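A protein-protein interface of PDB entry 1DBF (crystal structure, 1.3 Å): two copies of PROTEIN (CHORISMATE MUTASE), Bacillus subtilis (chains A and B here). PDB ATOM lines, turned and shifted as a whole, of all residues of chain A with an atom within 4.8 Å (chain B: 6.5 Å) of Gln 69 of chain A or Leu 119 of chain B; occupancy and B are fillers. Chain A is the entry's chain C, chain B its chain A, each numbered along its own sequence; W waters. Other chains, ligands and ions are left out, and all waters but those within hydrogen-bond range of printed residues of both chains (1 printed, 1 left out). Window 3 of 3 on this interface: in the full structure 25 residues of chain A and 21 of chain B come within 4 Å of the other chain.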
ATOM      1  N   ARG A  63      -3.317  -0.912 -18.236  1.00  0.00           N
ATOM      2  CA  ARG A  63      -4.651  -1.396 -17.915  1.00  0.00           C
ATOM      3  C   ARG A  63      -5.645  -0.937 -18.964  1.00  0.00           C
ATOM      4  O   ARG A  63      -6.707  -1.549 -19.162  1.00  0.00           O
ATOM      5  CB  ARG A  63      -5.058  -0.921 -16.522  1.00  0.00           C
ATOM      6  CG  ARG A  63      -4.097  -1.398 -15.444  1.00  0.00           C
ATOM      7  CD  ARG A  63      -4.691  -1.298 -14.031  1.00  0.00           C
ATOM      8  NE  ARG A  63      -3.675  -1.821 -13.113  1.00  0.00           N
ATOM      9  CZ  ARG A  63      -2.888  -1.122 -12.328  1.00  0.00           C
ATOM     10  NH1 ARG A  63      -2.923   0.204 -12.269  1.00  0.00           N
ATOM     11  NH2 ARG A  63      -2.029  -1.805 -11.587  1.00  0.00           N
ATOM     12  N   LEU A  65      -4.812  -0.457 -22.268  1.00  0.00           N
ATOM     13  CA  LEU A  65      -4.496  -0.934 -23.619  1.00  0.00           C
ATOM     14  C   LEU A  65      -5.377  -2.119 -24.002  1.00  0.00           C
ATOM     15  O   LEU A  65      -5.455  -3.112 -23.259  1.00  0.00           O
ATOM     16  CB  LEU A  65      -3.023  -1.379 -23.680  1.00  0.00           C
ATOM     17  CG  LEU A  65      -2.483  -1.541 -25.108  1.00  0.00           C
ATOM     18  CD1 LEU A  65      -2.409  -0.172 -25.784  1.00  0.00           C
ATOM     19  CD2 LEU A  65      -1.140  -2.248 -25.065  1.00  0.00           C
ATOM     20  N   SER A  66      -6.061  -2.058 -25.139  1.00  0.00           N
ATOM     21  CA  SER A  66      -6.977  -3.124 -25.541  1.00  0.00           C
ATOM     22  C   SER A  66      -6.331  -4.509 -25.481  1.00  0.00           C
ATOM     23  O   SER A  66      -5.274  -4.754 -26.052  1.00  0.00           O
ATOM     24  CB  SER A  66      -7.478  -2.859 -26.976  1.00  0.00           C
ATOM     25  OG  SER A  66      -8.142  -1.596 -26.978  1.00  0.00           O
ATOM     26  N   GLY A  67      -6.982  -5.408 -24.759  1.00  0.00           N
ATOM     27  CA  GLY A  67      -6.553  -6.769 -24.626  1.00  0.00           C
ATOM     28  C   GLY A  67      -5.543  -6.980 -23.514  1.00  0.00           C
ATOM     29  O   GLY A  67      -5.227  -8.153 -23.267  1.00  0.00           O
ATOM     30  N   TRP A  68      -5.066  -5.931 -22.864  1.00  0.00           N
ATOM     31  CA  TRP A  68      -4.056  -6.061 -21.798  1.00  0.00           C
ATOM     32  C   TRP A  68      -4.724  -5.948 -20.430  1.00  0.00           C
ATOM     33  O   TRP A  68      -4.002  -5.845 -19.419  1.00  0.00           O
ATOM     34  CB  TRP A  68      -2.946  -5.026 -22.060  1.00  0.00           C
ATOM     35  CG  TRP A  68      -2.056  -5.489 -23.185  1.00  0.00           C
ATOM     36  CD1 TRP A  68      -2.408  -5.667 -24.504  1.00  0.00           C
ATOM     37  CD2 TRP A  68      -0.663  -5.839 -23.094  1.00  0.00           C
ATOM     38  NE1 TRP A  68      -1.304  -6.102 -25.214  1.00  0.00           N
ATOM     39  CE2 TRP A  68      -0.237  -6.214 -24.372  1.00  0.00           C
ATOM     40  CE3 TRP A  68       0.264  -5.866 -22.020  1.00  0.00           C
ATOM     41  CZ2 TRP A  68       1.081  -6.619 -24.639  1.00  0.00           C
ATOM     42  CZ3 TRP A  68       1.605  -6.268 -22.254  1.00  0.00           C
ATOM     43  CH2 TRP A  68       1.947  -6.630 -23.573  1.00  0.00           C
ATOM     44  N   GLN A  69      -6.079  -5.960 -20.356  1.00  0.00           N
ATOM     45  CA  GLN A  69      -6.722  -5.644 -19.066  1.00  0.00           C
ATOM     46  C   GLN A  69      -6.586  -6.719 -17.981  1.00  0.00           C
ATOM     47  O   GLN A  69      -6.900  -6.463 -16.807  1.00  0.00           O
ATOM     48  CB  GLN A  69      -8.209  -5.306 -19.241  1.00  0.00           C
ATOM     49  CG  GLN A  69      -9.005  -6.480 -19.807  1.00  0.00           C
ATOM     50  CD  GLN A  69      -9.127  -6.459 -21.317  1.00  0.00           C
ATOM     51  OE1 GLN A  69      -8.153  -6.064 -21.990  1.00  0.00           O
ATOM     52  NE2 GLN A  69     -10.266  -6.831 -21.877  1.00  0.00           N
ATOM     53  N   TYR A  70      -6.094  -7.896 -18.380  1.00  0.00           N
ATOM     54  CA  TYR A  70      -5.815  -8.973 -17.446  1.00  0.00           C
ATOM     55  C   TYR A  70      -4.321  -9.177 -17.250  1.00  0.00           C
ATOM     56  O   TYR A  70      -3.868 -10.130 -16.586  1.00  0.00           O
ATOM     57  CB  TYR A  70      -6.468 -10.321 -17.863  1.00  0.00           C
ATOM     58  CG  TYR A  70      -7.979 -10.141 -17.910  1.00  0.00           C
ATOM     59  CD1 TYR A  70      -8.745 -10.156 -16.749  1.00  0.00           C
ATOM     60  CD2 TYR A  70      -8.630  -9.955 -19.117  1.00  0.00           C
ATOM     61  CE1 TYR A  70     -10.132  -9.995 -16.755  1.00  0.00           C
ATOM     62  CE2 TYR A  70     -10.020  -9.778 -19.146  1.00  0.00           C
ATOM     63  CZ  TYR A  70     -10.759  -9.814 -17.986  1.00  0.00           C
ATOM     64  OH  TYR A  70     -12.123  -9.615 -17.989  1.00  0.00           O
ATOM     65  N   VAL A  71      -3.479  -8.307 -17.808  1.00  0.00           N
ATOM     66  CA  VAL A  71      -2.029  -8.393 -17.520  1.00  0.00           C
ATOM     67  C   VAL A  71      -1.740  -7.821 -16.133  1.00  0.00           C
ATOM     68  O   VAL A  71      -1.940  -6.614 -15.961  1.00  0.00           O
ATOM     69  CB  VAL A  71      -1.179  -7.688 -18.579  1.00  0.00           C
ATOM     70  CG1 VAL A  71       0.299  -7.686 -18.236  1.00  0.00           C
ATOM     71  CG2 VAL A  71      -1.399  -8.331 -19.944  1.00  0.00           C
ATOM     72  N   GLN B 101      -5.016 -16.541 -17.654  1.00  0.00           N
ATOM     73  CA  GLN B 101      -4.813 -15.163 -17.205  1.00  0.00           C
ATOM     74  C   GLN B 101      -6.123 -14.493 -16.801  1.00  0.00           C
ATOM     75  O   GLN B 101      -6.126 -13.823 -15.746  1.00  0.00           O
ATOM     76  CB  GLN B 101      -4.073 -14.384 -18.310  1.00  0.00           C
ATOM     77  CG  GLN B 101      -3.778 -12.934 -17.973  1.00  0.00           C
ATOM     78  CD  GLN B 101      -3.040 -12.224 -19.092  1.00  0.00           C
ATOM     79  OE1 GLN B 101      -1.824 -12.054 -19.121  1.00  0.00           O
ATOM     80  NE2 GLN B 101      -3.848 -11.802 -20.065  1.00  0.00           N
ATOM     81  N   ARG B 116     -10.624  -1.768  -7.677  1.00  0.00           N
ATOM     82  CA  ARG B 116     -10.904  -2.915  -8.529  1.00  0.00           C
ATOM     83  C   ARG B 116     -11.365  -2.427  -9.900  1.00  0.00           C
ATOM     84  O   ARG B 116     -12.018  -1.385 -10.051  1.00  0.00           O
ATOM     85  CB  ARG B 116     -11.903  -3.829  -7.844  1.00  0.00           C
ATOM     86  CG  ARG B 116     -13.281  -3.277  -7.736  1.00  0.00           C
ATOM     87  CD  ARG B 116     -14.246  -4.199  -6.980  1.00  0.00           C
ATOM     88  NE  ARG B 116     -14.425  -5.469  -7.691  1.00  0.00           N
ATOM     89  CZ  ARG B 116     -15.371  -6.358  -7.410  1.00  0.00           C
ATOM     90  NH1 ARG B 116     -16.237  -6.110  -6.428  1.00  0.00           N
ATOM     91  NH2 ARG B 116     -15.488  -7.494  -8.078  1.00  0.00           N
ATOM     92  N   PRO B 117     -10.964  -3.110 -10.958  1.00  0.00           N
ATOM     93  CA  PRO B 117     -11.232  -2.616 -12.337  1.00  0.00           C
ATOM     94  C   PRO B 117     -12.657  -2.876 -12.794  1.00  0.00           C
ATOM     95  O   PRO B 117     -13.076  -2.293 -13.810  1.00  0.00           O
ATOM     96  CB  PRO B 117     -10.211  -3.403 -13.176  1.00  0.00           C
ATOM     97  CG  PRO B 117     -10.145  -4.711 -12.463  1.00  0.00           C
ATOM     98  CD  PRO B 117     -10.175  -4.335 -10.992  1.00  0.00           C
ATOM     99  N   ASP B 118     -13.431  -3.707 -12.090  1.00  0.00           N
ATOM    100  CA  ASP B 118     -14.823  -3.965 -12.500  1.00  0.00           C
ATOM    101  C   ASP B 118     -14.963  -4.388 -13.947  1.00  0.00           C
ATOM    102  O   ASP B 118     -15.789  -3.844 -14.708  1.00  0.00           O
ATOM    103  CB  ASP B 118     -15.701  -2.717 -12.331  1.00  0.00           C
ATOM    104  CG  ASP B 118     -15.768  -2.377 -10.841  1.00  0.00           C
ATOM    105  OD1 ASP B 118     -15.722  -3.361 -10.064  1.00  0.00           O
ATOM    106  OD2 ASP B 118     -15.897  -1.172 -10.515  1.00  0.00           O
ATOM    107  N   LEU B 119     -14.159  -5.368 -14.330  1.00  0.00           N
ATOM    108  CA  LEU B 119     -14.161  -5.844 -15.698  1.00  0.00           C
ATOM    109  C   LEU B 119     -15.368  -6.740 -15.912  1.00  0.00           C
ATOM    110  O   LEU B 119     -15.875  -7.335 -14.953  1.00  0.00           O
ATOM    111  CB  LEU B 119     -12.834  -6.577 -15.976  1.00  0.00           C
ATOM    112  CG  LEU B 119     -11.609  -5.689 -15.797  1.00  0.00           C
ATOM    113  CD1 LEU B 119     -10.303  -6.475 -15.809  1.00  0.00           C
ATOM    114  CD2 LEU B 119     -11.573  -4.618 -16.889  1.00  0.00           C
ATOM    115  N   SER B 120     -15.792  -6.843 -17.181  1.00  0.00           N
ATOM    116  CA  SER B 120     -16.886  -7.741 -17.496  1.00  0.00           C
ATOM    117  C   SER B 120     -16.455  -8.767 -18.513  1.00  0.00           C
ATOM    118  O   SER B 120     -16.415  -8.479 -19.701  1.00  0.00           O
ATOM    119  CB  SER B 120     -18.079  -6.977 -18.081  1.00  0.00           C
ATOM    120  OG  SER B 120     -19.054  -7.916 -18.572  1.00  0.00           O
ATOM    121  N   LEU B 121     -16.120  -9.959 -18.044  1.00  0.00           N
ATOM    122  CA  LEU B 121     -15.709 -10.979 -19.013  1.00  0.00           C
ATOM    123  C   LEU B 121     -16.950 -11.478 -19.740  1.00  0.00           C
ATOM    124  O   LEU B 121     -16.875 -11.935 -20.884  1.00  0.00           O
ATOM    125  CB  LEU B 121     -14.939 -12.015 -18.199  1.00  0.00           C
ATOM    126  CG  LEU B 121     -14.038 -13.031 -18.866  1.00  0.00           C
ATOM    127  CD1 LEU B 121     -13.091 -12.383 -19.859  1.00  0.00           C
ATOM    128  CD2 LEU B 121     -13.312 -13.847 -17.782  1.00  0.00           C
ATOM    129  N   THR B 122     -18.121 -11.369 -19.088  1.00  0.00           N
ATOM    130  CA  THR B 122     -19.345 -11.864 -19.737  1.00  0.00           C
ATOM    131  C   THR B 122     -19.527 -11.096 -21.022  1.00  0.00           C
ATOM    132  O   THR B 122     -19.917 -11.575 -22.085  1.00  0.00           O
ATOM    133  CB  THR B 122     -20.548 -11.705 -18.792  1.00  0.00           C
ATOM    134  OG1 THR B 122     -20.502 -12.709 -17.756  1.00  0.00           O
ATOM    135  CG2 THR B 122     -21.895 -11.945 -19.455  1.00  0.00           C
ATOM    136  N   ASN B 124     -16.883  -9.137 -22.456  1.00  0.00           N
ATOM    137  CA  ASN B 124     -15.623  -9.082 -23.222  1.00  0.00           C
ATOM    138  C   ASN B 124     -15.422 -10.330 -24.097  1.00  0.00           C
ATOM    139  O   ASN B 124     -14.765 -10.221 -25.130  1.00  0.00           O
ATOM    140  CB  ASN B 124     -14.407  -8.838 -22.324  1.00  0.00           C
ATOM    141  CG  ASN B 124     -13.212  -8.374 -23.156  1.00  0.00           C
ATOM    142  OD1 ASN B 124     -13.132  -7.237 -23.627  1.00  0.00           O
ATOM    143  ND2 ASN B 124     -12.235  -9.262 -23.348  1.00  0.00           N
HETATM  144  O   HOH W   1      -4.342 -11.975 -14.741  1.00  0.00           O
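OD1 of Asn 124 of chain B lies within hydrogen-bond range of NE2 of Gln 69 of chain A.
OE1 of Gln 69 of chain A sits at hydrogen-bond distance from N of Gly 67 of chain A (3.1 Å).
Among the printed residues, pairs that only touch across the chains: Gln 69 of chain A with Leu 119 of chain B, Tyr 70 of chain A with Gln 101 of chain B, Tyr 70 of chain A with Leu 119 of chain B, Tyr 70 of chain A with Leu 121 of chain B and Val 71 of chain A with Gln 101 of chain B.
Leu 65 of chain A touches none of the printed residues of chain B.
Gln 69 of chain A touches just these residues of chain B: Leu 119 and Asn 124.
Of the printed residues of chain B, Tyr 70 of chain A touches Gln 101 (3.1 Å), Leu 119 (3.6 Å) and Leu 121 (3.5 Å).
Printed residues of chain A within 4 Å of Gln 101 of chain B: Tyr 70 and Val 71.
Leu 119 of chain B touches just these residues of chain A: Gln 69 (3.5 Å) and Tyr 70 (3.6 Å).
Printed residues of chain A within 4 Å of Leu 121 of chain B: Tyr 70.
The nearest printed residue of chain A that does not touch Gln 101 of chain B is Gly 67 of chain A (5.0 Å).
Printed residues of chain A that touch a printed residue of chain B: Gln 69, Tyr 70 and Val 71.
Hydrophobic or aromatic side chains of chain A that line the printed part of chain B: Tyr 70 and Val 71.
Among the printed residues, 6 pairs touch across the chains.
No position is printed for both chains.
Of the 6 pairs that touch across the chains among the printed residues, none has its exchanged pair printed and touching as well.
Water W1 bridges the backbone carbonyl oxygen (O) of Tyr 70 of chain A and the backbone carbonyl oxygen (O) of Gln 101 of chain B.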
